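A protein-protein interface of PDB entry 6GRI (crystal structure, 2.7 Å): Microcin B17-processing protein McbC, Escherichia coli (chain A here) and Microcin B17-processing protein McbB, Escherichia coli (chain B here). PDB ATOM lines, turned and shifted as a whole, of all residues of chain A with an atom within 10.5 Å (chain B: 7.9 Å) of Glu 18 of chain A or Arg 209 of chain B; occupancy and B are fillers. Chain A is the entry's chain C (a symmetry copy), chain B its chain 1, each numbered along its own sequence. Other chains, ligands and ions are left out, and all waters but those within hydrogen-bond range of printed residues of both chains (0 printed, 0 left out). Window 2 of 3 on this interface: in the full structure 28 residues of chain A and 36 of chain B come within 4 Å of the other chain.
Glu 18 of chain A touches just these residues of chain B: Arg 209 (3.5 Å), Arg 210 (2.8 Å) and Asn 211 (3.3 Å). Of chain A, only Glu 18 (3.5 Å) comes within 4 Å of Arg 209 of chain B. Of the printed residues of chain B, Pro 17 of chain A touches Asn 211. Phe 208 of chain B touches none of the printed residues of chain A. Asn 211 of chain B touches just these residues of chain A: Pro 17 and Glu 18. Of the printed residues of chain B, Ala 21 of chain A touches Arg 210 (3.6 Å). Of the printed residues of chain B, Ile 22 of chain A touches Arg 210 (3.99 Å). Printed residues of chain A within 4 Å of Arg 210 of chain B: Glu 18 (2.8 Å), Ala 21 (3.6 Å), Ile 22 (3.99 Å) and Asp 25 (2.6 Å). Of the printed residues of chain A, Arg 199 of chain B touches Asp 25 (3.3 Å). Tyr 14 of chain A touches none of the printed residues of chain B.
The guanidinium group (NE) of Arg 210 of chain B lies within salt-bridge range of the side-chain carboxylate (OD2) of Asp 25 of chain A. The side-chain carboxylate of Asp 25 of chain A lies within salt-bridge range of the guanidinium group of Arg 199 of chain B, at 3.3 Å. The backbone NH (N) of Arg 210 of chain B sits at hydrogen-bond distance from the side-chain carboxylate (OE1) of Glu 18 of chain A (2.8 Å). N of Asn 211 of chain B lies within hydrogen-bond range of OE1 of Glu 18 of chain A.
Of the 12 printed residues of chain B, 4 touch a printed residue of chain A. Of the 17 printed residues of chain A, 5 touch a printed residue of chain B. Hydrophobic or aromatic side chains of chain A that line the printed part of chain B: Pro 17, Ala 21 and Ile 22. Among the printed residues, 8 pairs touch across the chains. Among the printed residues, Asp or Glu carboxylates within 4 Å of a Lys or Arg side-chain nitrogen of the other chain: Asp 25 of chain A with Arg 199 of chain B (3.3 Å) and Asp 25 of chain A with Arg 210 of chain B (2.6 Å).
Among the printed residues, pairs that only touch across the chains: Glu 18 of chain A with Arg 209 of chain B, Ala 21 of chain A with Arg 210 of chain B, Pro 17 of chain A with Asn 211 of chain B and Ile 22 of chain A with Arg 210 of chain B.
The backbone carbonyl oxygen (O) of Arg 199 of chain B sits at hydrogen-bond distance from the side-chain hydroxyl (OG) of Ser 202 of chain B, 3.0 Å away. The backbone carbonyl oxygen (O) of Arg 209 of chain B sits at hydrogen-bond distance from the side-chain hydroxyl (OG) of Ser 207 of chain B (3.0 Å). OD1 of Asp 16 of chain A sits at hydrogen-bond distance from N of Glu 18 of chain A (2.9 Å).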
ATOM      1  N   TYR A  14     -13.505  -1.865 -21.490  1.00  0.00           N
ATOM      2  CA  TYR A  14     -12.947  -0.623 -20.933  1.00  0.00           C
ATOM      3  C   TYR A  14     -11.669  -0.165 -21.641  1.00  0.00           C
ATOM      4  O   TYR A  14     -10.963   0.715 -21.144  1.00  0.00           O
ATOM      5  CB  TYR A  14     -12.634  -0.818 -19.444  1.00  0.00           C
ATOM      6  CG  TYR A  14     -13.854  -1.067 -18.598  1.00  0.00           C
ATOM      7  CD1 TYR A  14     -14.540  -0.005 -18.020  1.00  0.00           C
ATOM      8  CD2 TYR A  14     -14.328  -2.369 -18.366  1.00  0.00           C
ATOM      9  CE1 TYR A  14     -15.660  -0.223 -17.247  1.00  0.00           C
ATOM     10  CE2 TYR A  14     -15.453  -2.589 -17.590  1.00  0.00           C
ATOM     11  CZ  TYR A  14     -16.115  -1.513 -17.042  1.00  0.00           C
ATOM     12  OH  TYR A  14     -17.230  -1.696 -16.274  1.00  0.00           O
ATOM     13  N   THR A  15     -11.363  -0.748 -22.792  1.00  0.00           N
ATOM     14  CA  THR A  15     -10.092  -0.499 -23.446  1.00  0.00           C
ATOM     15  C   THR A  15     -10.121   0.780 -24.242  1.00  0.00           C
ATOM     16  O   THR A  15     -10.964   0.953 -25.116  1.00  0.00           O
ATOM     17  CB  THR A  15      -9.735  -1.645 -24.396  1.00  0.00           C
ATOM     18  OG1 THR A  15      -9.583  -2.840 -23.630  1.00  0.00           O
ATOM     19  CG2 THR A  15      -8.431  -1.344 -25.178  1.00  0.00           C
ATOM     20  N   ASP A  16      -9.182   1.667 -23.951  1.00  0.00           N
ATOM     21  CA  ASP A  16      -8.942   2.820 -24.805  1.00  0.00           C
ATOM     22  C   ASP A  16      -8.041   2.347 -25.941  1.00  0.00           C
ATOM     23  O   ASP A  16      -6.912   1.909 -25.700  1.00  0.00           O
ATOM     24  CB  ASP A  16      -8.282   3.960 -24.028  1.00  0.00           C
ATOM     25  CG  ASP A  16      -8.193   5.230 -24.836  1.00  0.00           C
ATOM     26  OD1 ASP A  16      -8.008   5.154 -26.068  1.00  0.00           O
ATOM     27  OD2 ASP A  16      -8.306   6.310 -24.232  1.00  0.00           O
ATOM     28  N   PRO A  17      -8.538   2.408 -27.178  1.00  0.00           N
ATOM     29  CA  PRO A  17      -7.734   1.927 -28.298  1.00  0.00           C
ATOM     30  C   PRO A  17      -6.571   2.852 -28.706  1.00  0.00           C
ATOM     31  O   PRO A  17      -5.594   2.367 -29.272  1.00  0.00           O
ATOM     32  CB  PRO A  17      -8.757   1.778 -29.418  1.00  0.00           C
ATOM     33  CG  PRO A  17      -9.827   2.752 -29.084  1.00  0.00           C
ATOM     34  CD  PRO A  17      -9.867   2.874 -27.601  1.00  0.00           C
ATOM     35  N   GLU A  18      -6.669   4.157 -28.436  1.00  0.00           N
ATOM     36  CA  GLU A  18      -5.521   5.069 -28.579  1.00  0.00           C
ATOM     37  C   GLU A  18      -4.412   4.619 -27.637  1.00  0.00           C
ATOM     38  O   GLU A  18      -3.256   4.530 -28.046  1.00  0.00           O
ATOM     39  CB  GLU A  18      -5.910   6.518 -28.272  1.00  0.00           C
ATOM     40  CG  GLU A  18      -4.785   7.565 -28.329  1.00  0.00           C
ATOM     41  CD  GLU A  18      -4.564   8.204 -29.699  1.00  0.00           C
ATOM     42  OE1 GLU A  18      -5.242   7.846 -30.694  1.00  0.00           O
ATOM     43  OE2 GLU A  18      -3.688   9.088 -29.782  1.00  0.00           O
ATOM     44  N   VAL A  19      -4.755   4.308 -26.389  1.00  0.00           N
ATOM     45  CA  VAL A  19      -3.732   3.864 -25.442  1.00  0.00           C
ATOM     46  C   VAL A  19      -3.102   2.554 -25.908  1.00  0.00           C
ATOM     47  O   VAL A  19      -1.874   2.388 -25.827  1.00  0.00           O
ATOM     48  CB  VAL A  19      -4.259   3.699 -24.010  1.00  0.00           C
ATOM     49  CG1 VAL A  19      -3.166   3.155 -23.102  1.00  0.00           C
ATOM     50  CG2 VAL A  19      -4.771   5.022 -23.467  1.00  0.00           C
ATOM     51  N   LEU A  20      -3.933   1.631 -26.397  1.00  0.00           N
ATOM     52  CA  LEU A  20      -3.450   0.290 -26.729  1.00  0.00           C
ATOM     53  C   LEU A  20      -2.459   0.359 -27.875  1.00  0.00           C
ATOM     54  O   LEU A  20      -1.384  -0.224 -27.803  1.00  0.00           O
ATOM     55  CB  LEU A  20      -4.613  -0.613 -27.103  1.00  0.00           C
ATOM     56  CG  LEU A  20      -4.302  -2.077 -27.383  1.00  0.00           C
ATOM     57  CD1 LEU A  20      -3.839  -2.796 -26.116  1.00  0.00           C
ATOM     58  CD2 LEU A  20      -5.529  -2.743 -27.981  1.00  0.00           C
ATOM     59  N   ALA A  21      -2.832   1.080 -28.926  1.00  0.00           N
ATOM     60  CA  ALA A  21      -1.965   1.283 -30.087  1.00  0.00           C
ATOM     61  C   ALA A  21      -0.601   1.893 -29.724  1.00  0.00           C
ATOM     62  O   ALA A  21       0.426   1.414 -30.185  1.00  0.00           O
ATOM     63  CB  ALA A  21      -2.667   2.170 -31.098  1.00  0.00           C
ATOM     64  N   ILE A  22      -0.615   2.946 -28.906  1.00  0.00           N
ATOM     65  CA  ILE A  22       0.599   3.671 -28.492  1.00  0.00           C
ATOM     66  C   ILE A  22       1.555   2.827 -27.612  1.00  0.00           C
ATOM     67  O   ILE A  22       2.777   2.910 -27.765  1.00  0.00           O
ATOM     68  CB  ILE A  22       0.201   5.019 -27.820  1.00  0.00           C
ATOM     69  CG1 ILE A  22      -0.185   6.022 -28.910  1.00  0.00           C
ATOM     70  CG2 ILE A  22       1.318   5.596 -26.966  1.00  0.00           C
ATOM     71  CD1 ILE A  22      -1.015   7.180 -28.413  1.00  0.00           C
ATOM     72  N   VAL A  23       0.994   2.007 -26.721  1.00  0.00           N
ATOM     73  CA  VAL A  23       1.779   1.090 -25.885  1.00  0.00           C
ATOM     74  C   VAL A  23       2.416  -0.013 -26.727  1.00  0.00           C
ATOM     75  O   VAL A  23       3.579  -0.352 -26.513  1.00  0.00           O
ATOM     76  CB  VAL A  23       0.914   0.457 -24.775  1.00  0.00           C
ATOM     77  CG1 VAL A  23       1.687  -0.592 -23.992  1.00  0.00           C
ATOM     78  CG2 VAL A  23       0.394   1.523 -23.818  1.00  0.00           C
ATOM     79  N   LYS A  24       1.652  -0.583 -27.662  1.00  0.00           N
ATOM     80  CA  LYS A  24       2.165  -1.615 -28.568  1.00  0.00           C
ATOM     81  C   LYS A  24       3.260  -1.082 -29.498  1.00  0.00           C
ATOM     82  O   LYS A  24       4.294  -1.722 -29.633  1.00  0.00           O
ATOM     83  CB  LYS A  24       1.044  -2.197 -29.425  1.00  0.00           C
ATOM     84  CG  LYS A  24       0.089  -3.158 -28.733  1.00  0.00           C
ATOM     85  CD  LYS A  24      -1.075  -3.435 -29.670  1.00  0.00           C
ATOM     86  CE  LYS A  24      -1.793  -4.722 -29.326  1.00  0.00           C
ATOM     87  NZ  LYS A  24      -2.734  -5.123 -30.410  1.00  0.00           N
ATOM     88  N   ASP A  25       3.023   0.072 -30.137  1.00  0.00           N
ATOM     89  CA  ASP A  25       4.046   0.777 -30.963  1.00  0.00           C
ATOM     90  C   ASP A  25       5.366   0.976 -30.240  1.00  0.00           C
ATOM     91  O   ASP A  25       6.420   0.943 -30.873  1.00  0.00           O
ATOM     92  CB  ASP A  25       3.604   2.176 -31.366  1.00  0.00           C
ATOM     93  CG  ASP A  25       2.424   2.190 -32.304  1.00  0.00           C
ATOM     94  OD1 ASP A  25       1.963   1.113 -32.749  1.00  0.00           O
ATOM     95  OD2 ASP A  25       1.943   3.313 -32.595  1.00  0.00           O
ATOM     96  N   PHE A  26       5.292   1.235 -28.930  1.00  0.00           N
ATOM     97  CA  PHE A  26       6.477   1.443 -28.109  1.00  0.00           C
ATOM     98  C   PHE A  26       7.110   0.117 -27.808  1.00  0.00           C
ATOM     99  O   PHE A  26       8.280  -0.082 -28.061  1.00  0.00           O
ATOM    100  CB  PHE A  26       6.146   2.171 -26.793  1.00  0.00           C
ATOM    101  CG  PHE A  26       7.326   2.318 -25.889  1.00  0.00           C
ATOM    102  CD1 PHE A  26       8.322   3.226 -26.186  1.00  0.00           C
ATOM    103  CD2 PHE A  26       7.472   1.512 -24.775  1.00  0.00           C
ATOM    104  CE1 PHE A  26       9.440   3.353 -25.376  1.00  0.00           C
ATOM    105  CE2 PHE A  26       8.590   1.632 -23.954  1.00  0.00           C
ATOM    106  CZ  PHE A  26       9.578   2.556 -24.262  1.00  0.00           C
ATOM    107  N   GLU A 196      -4.199  -5.655 -23.047  1.00  0.00           N
ATOM    108  CA  GLU A 196      -5.504  -5.082 -22.678  1.00  0.00           C
ATOM    109  C   GLU A 196      -5.850  -5.205 -21.185  1.00  0.00           C
ATOM    110  O   GLU A 196      -6.492  -4.313 -20.625  1.00  0.00           O
ATOM    111  CB  GLU A 196      -6.623  -5.663 -23.548  1.00  0.00           C
ATOM    112  CG  GLU A 196      -6.505  -5.257 -25.021  1.00  0.00           C
ATOM    113  CD  GLU A 196      -7.841  -5.177 -25.752  1.00  0.00           C
ATOM    114  OE1 GLU A 196      -8.837  -4.690 -25.179  1.00  0.00           O
ATOM    115  OE2 GLU A 196      -7.888  -5.595 -26.926  1.00  0.00           O
ATOM    116  N   LEU A 199      -3.690  -2.534 -19.386  1.00  0.00           N
ATOM    117  CA  LEU A 199      -4.003  -1.125 -19.653  1.00  0.00           C
ATOM    118  C   LEU A 199      -5.415  -0.641 -19.280  1.00  0.00           C
ATOM    119  O   LEU A 199      -5.642   0.577 -19.152  1.00  0.00           O
ATOM    120  CB  LEU A 199      -3.735  -0.838 -21.134  1.00  0.00           C
ATOM    121  CG  LEU A 199      -2.284  -1.051 -21.585  1.00  0.00           C
ATOM    122  CD1 LEU A 199      -2.217  -1.130 -23.099  1.00  0.00           C
ATOM    123  CD2 LEU A 199      -1.360   0.043 -21.051  1.00  0.00           C
ATOM    124  N   ARG A 203      -4.580   2.774 -17.546  1.00  0.00           N
ATOM    125  CA  ARG A 203      -4.060   3.328 -18.803  1.00  0.00           C
ATOM    126  C   ARG A 203      -2.540   3.123 -18.893  1.00  0.00           C
ATOM    127  O   ARG A 203      -2.052   2.077 -18.477  1.00  0.00           O
ATOM    128  CB  ARG A 203      -4.505   4.786 -18.988  1.00  0.00           C
ATOM    129  CG  ARG A 203      -6.007   4.957 -18.935  1.00  0.00           C
ATOM    130  CD  ARG A 203      -6.408   6.411 -18.857  1.00  0.00           C
ATOM    131  NE  ARG A 203      -5.823   7.194 -19.936  1.00  0.00           N
ATOM    132  CZ  ARG A 203      -6.258   7.235 -21.190  1.00  0.00           C
ATOM    133  NH1 ARG A 203      -7.304   6.528 -21.597  1.00  0.00           N
ATOM    134  NH2 ARG A 203      -5.619   7.994 -22.056  1.00  0.00           N
ATOM    135  N   TYR A 204      -1.802   4.111 -19.393  1.00  0.00           N
ATOM    136  CA  TYR A 204      -0.352   3.992 -19.640  1.00  0.00           C
ATOM    137  C   TYR A 204       0.456   3.488 -18.447  1.00  0.00           C
ATOM    138  O   TYR A 204       1.354   2.684 -18.608  1.00  0.00           O
ATOM    139  CB  TYR A 204       0.209   5.336 -20.110  1.00  0.00           C
ATOM    140  CG  TYR A 204      -0.321   5.751 -21.458  1.00  0.00           C
ATOM    141  CD1 TYR A 204       0.084   5.087 -22.610  1.00  0.00           C
ATOM    142  CD2 TYR A 204      -1.247   6.785 -21.581  1.00  0.00           C
ATOM    143  CE1 TYR A 204      -0.396   5.462 -23.853  1.00  0.00           C
ATOM    144  CE2 TYR A 204      -1.742   7.166 -22.821  1.00  0.00           C
ATOM    145  CZ  TYR A 204      -1.315   6.497 -23.947  1.00  0.00           C
ATOM    146  OH  TYR A 204      -1.800   6.843 -25.175  1.00  0.00           O
ATOM    147  N   ARG B 199      -0.720   0.814 -41.096  1.00  0.00           N
ATOM    148  CA  ARG B 199       0.063   1.771 -40.302  1.00  0.00           C
ATOM    149  C   ARG B 199       0.218   3.098 -41.044  1.00  0.00           C
ATOM    150  O   ARG B 199      -0.014   4.163 -40.467  1.00  0.00           O
ATOM    151  CB  ARG B 199       1.450   1.207 -39.954  1.00  0.00           C
ATOM    152  CG  ARG B 199       2.237   2.006 -38.928  1.00  0.00           C
ATOM    153  CD  ARG B 199       1.700   1.790 -37.525  1.00  0.00           C
ATOM    154  NE  ARG B 199       2.251   2.738 -36.552  1.00  0.00           N
ATOM    155  CZ  ARG B 199       1.935   4.036 -36.460  1.00  0.00           C
ATOM    156  NH1 ARG B 199       1.061   4.615 -37.292  1.00  0.00           N
ATOM    157  NH2 ARG B 199       2.507   4.774 -35.521  1.00  0.00           N
ATOM    158  N   SER B 202      -3.358   5.142 -41.781  1.00  0.00           N
ATOM    159  CA  SER B 202      -3.817   5.835 -40.575  1.00  0.00           C
ATOM    160  C   SER B 202      -2.968   7.077 -40.387  1.00  0.00           C
ATOM    161  O   SER B 202      -3.492   8.178 -40.308  1.00  0.00           O
ATOM    162  CB  SER B 202      -3.748   4.955 -39.317  1.00  0.00           C
ATOM    163  OG  SER B 202      -2.425   4.816 -38.820  1.00  0.00           O
ATOM    164  N   ARG B 203      -1.652   6.900 -40.375  1.00  0.00           N
ATOM    165  CA  ARG B 203      -0.737   8.030 -40.203  1.00  0.00           C
ATOM    166  C   ARG B 203      -1.007   9.198 -41.171  1.00  0.00           C
ATOM    167  O   ARG B 203      -0.931  10.352 -40.763  1.00  0.00           O
ATOM    168  CB  ARG B 203       0.722   7.577 -40.304  1.00  0.00           C
ATOM    169  CG  ARG B 203       1.723   8.668 -39.954  1.00  0.00           C
ATOM    170  CD  ARG B 203       3.148   8.149 -39.997  1.00  0.00           C
ATOM    171  NE  ARG B 203       3.513   7.442 -38.773  1.00  0.00           N
ATOM    172  CZ  ARG B 203       4.563   6.627 -38.635  1.00  0.00           C
ATOM    173  NH1 ARG B 203       5.395   6.390 -39.649  1.00  0.00           N
ATOM    174  NH2 ARG B 203       4.781   6.039 -37.462  1.00  0.00           N
ATOM    175  N   GLU B 205      -3.816  10.214 -42.545  1.00  0.00           N
ATOM    176  CA  GLU B 205      -5.111  10.898 -42.402  1.00  0.00           C
ATOM    177  C   GLU B 205      -5.079  11.981 -41.318  1.00  0.00           C
ATOM    178  O   GLU B 205      -4.315  11.877 -40.358  1.00  0.00           O
ATOM    179  CB  GLU B 205      -6.255   9.885 -42.168  1.00  0.00           C
ATOM    180  CG  GLU B 205      -7.163   9.638 -43.377  1.00  0.00           C
ATOM    181  CD  GLU B 205      -6.423   9.526 -44.710  1.00  0.00           C
ATOM    182  OE1 GLU B 205      -6.708  10.362 -45.596  1.00  0.00           O
ATOM    183  OE2 GLU B 205      -5.558   8.625 -44.873  1.00  0.00           O
ATOM    184  N   LYS B 206      -5.907  13.016 -41.504  1.00  0.00           N
ATOM    185  CA  LYS B 206      -5.992  14.155 -40.584  1.00  0.00           C
ATOM    186  C   LYS B 206      -6.981  13.845 -39.463  1.00  0.00           C
ATOM    187  O   LYS B 206      -8.128  14.305 -39.473  1.00  0.00           O
ATOM    188  CB  LYS B 206      -6.398  15.433 -41.330  1.00  0.00           C
ATOM    189  N   SER B 207      -6.513  13.032 -38.517  1.00  0.00           N
ATOM    190  CA  SER B 207      -7.257  12.656 -37.308  1.00  0.00           C
ATOM    191  C   SER B 207      -6.681  13.253 -36.011  1.00  0.00           C
ATOM    192  O   SER B 207      -7.439  13.454 -35.057  1.00  0.00           O
ATOM    193  CB  SER B 207      -7.297  11.130 -37.180  1.00  0.00           C
ATOM    194  OG  SER B 207      -5.985  10.591 -37.134  1.00  0.00           O
ATOM    195  N   PHE B 208      -5.366  13.529 -35.979  1.00  0.00           N
ATOM    196  CA  PHE B 208      -4.624  13.902 -34.749  1.00  0.00           C
ATOM    197  C   PHE B 208      -4.760  12.830 -33.647  1.00  0.00           C
ATOM    198  O   PHE B 208      -4.775  13.146 -32.442  1.00  0.00           O
ATOM    199  CB  PHE B 208      -5.044  15.293 -34.241  1.00  0.00           C
ATOM    200  N   ARG B 209      -4.837  11.569 -34.092  1.00  0.00           N
ATOM    201  CA  ARG B 209      -5.124  10.405 -33.245  1.00  0.00           C
ATOM    202  C   ARG B 209      -4.483   9.159 -33.874  1.00  0.00           C
ATOM    203  O   ARG B 209      -4.572   8.953 -35.087  1.00  0.00           O
ATOM    204  CB  ARG B 209      -6.641  10.210 -33.089  1.00  0.00           C
ATOM    205  N   ARG B 210      -3.832   8.346 -33.045  1.00  0.00           N
ATOM    206  CA  ARG B 210      -3.089   7.156 -33.500  1.00  0.00           C
ATOM    207  C   ARG B 210      -4.006   6.035 -34.019  1.00  0.00           C
ATOM    208  O   ARG B 210      -3.787   5.489 -35.112  1.00  0.00           O
ATOM    209  CB  ARG B 210      -2.198   6.633 -32.358  1.00  0.00           C
ATOM    210  CG  ARG B 210      -1.593   5.247 -32.557  1.00  0.00           C
ATOM    211  CD  ARG B 210      -0.700   5.189 -33.767  1.00  0.00           C
ATOM    212  NE  ARG B 210      -0.229   3.831 -33.990  1.00  0.00           N
ATOM    213  CZ  ARG B 210      -0.881   2.888 -34.663  1.00  0.00           C
ATOM    214  NH1 ARG B 210      -2.065   3.132 -35.213  1.00  0.00           N
ATOM    215  NH2 ARG B 210      -0.331   1.685 -34.791  1.00  0.00           N
ATOM    216  N   ASN B 211      -4.998   5.681 -33.208  1.00  0.00           N
ATOM    217  CA  ASN B 211      -6.000   4.690 -33.583  1.00  0.00           C
ATOM    218  C   ASN B 211      -6.918   5.274 -34.662  1.00  0.00           C
ATOM    219  O   ASN B 211      -7.540   6.315 -34.443  1.00  0.00           O
ATOM    220  CB  ASN B 211      -6.800   4.246 -32.350  1.00  0.00           C
ATOM    221  CG  ASN B 211      -8.220   3.842 -32.680  1.00  0.00           C
ATOM    222  OD1 ASN B 211      -8.510   2.664 -32.891  1.00  0.00           O
ATOM    223  ND2 ASN B 211      -9.115   4.826 -32.735  1.00  0.00           N
ATOM    224  N   GLU B 212      -7.009   4.584 -35.804  1.00  0.00           N
ATOM    225  CA  GLU B 212      -7.768   5.049 -36.977  1.00  0.00           C
ATOM    226  C   GLU B 212      -9.119   4.328 -37.138  1.00  0.00           C
ATOM    227  O   GLU B 212      -9.388   3.765 -38.207  1.00  0.00           O
ATOM    228  CB  GLU B 212      -6.924   4.836 -38.240  1.00  0.00           C
ATOM    229  N   MET B 213      -9.967   4.365 -36.100  1.00  0.00           N
ATOM    230  CA  MET B 213     -11.205   3.559 -36.066  1.00  0.00           C
ATOM    231  C   MET B 213     -12.450   4.330 -35.618  1.00  0.00           C
ATOM    232  O   MET B 213     -12.592   4.708 -34.462  1.00  0.00           O
ATOM    233  CB  MET B 213     -11.031   2.327 -35.171  1.00  0.00           C
ATOM    234  CG  MET B 213     -10.220   1.202 -35.791  1.00  0.00           C
ATOM    235  SD  MET B 213     -11.149   0.289 -37.032  1.00  0.00           S
ATOM    236  CE  MET B 213      -9.977  -1.009 -37.450  1.00  0.00           C
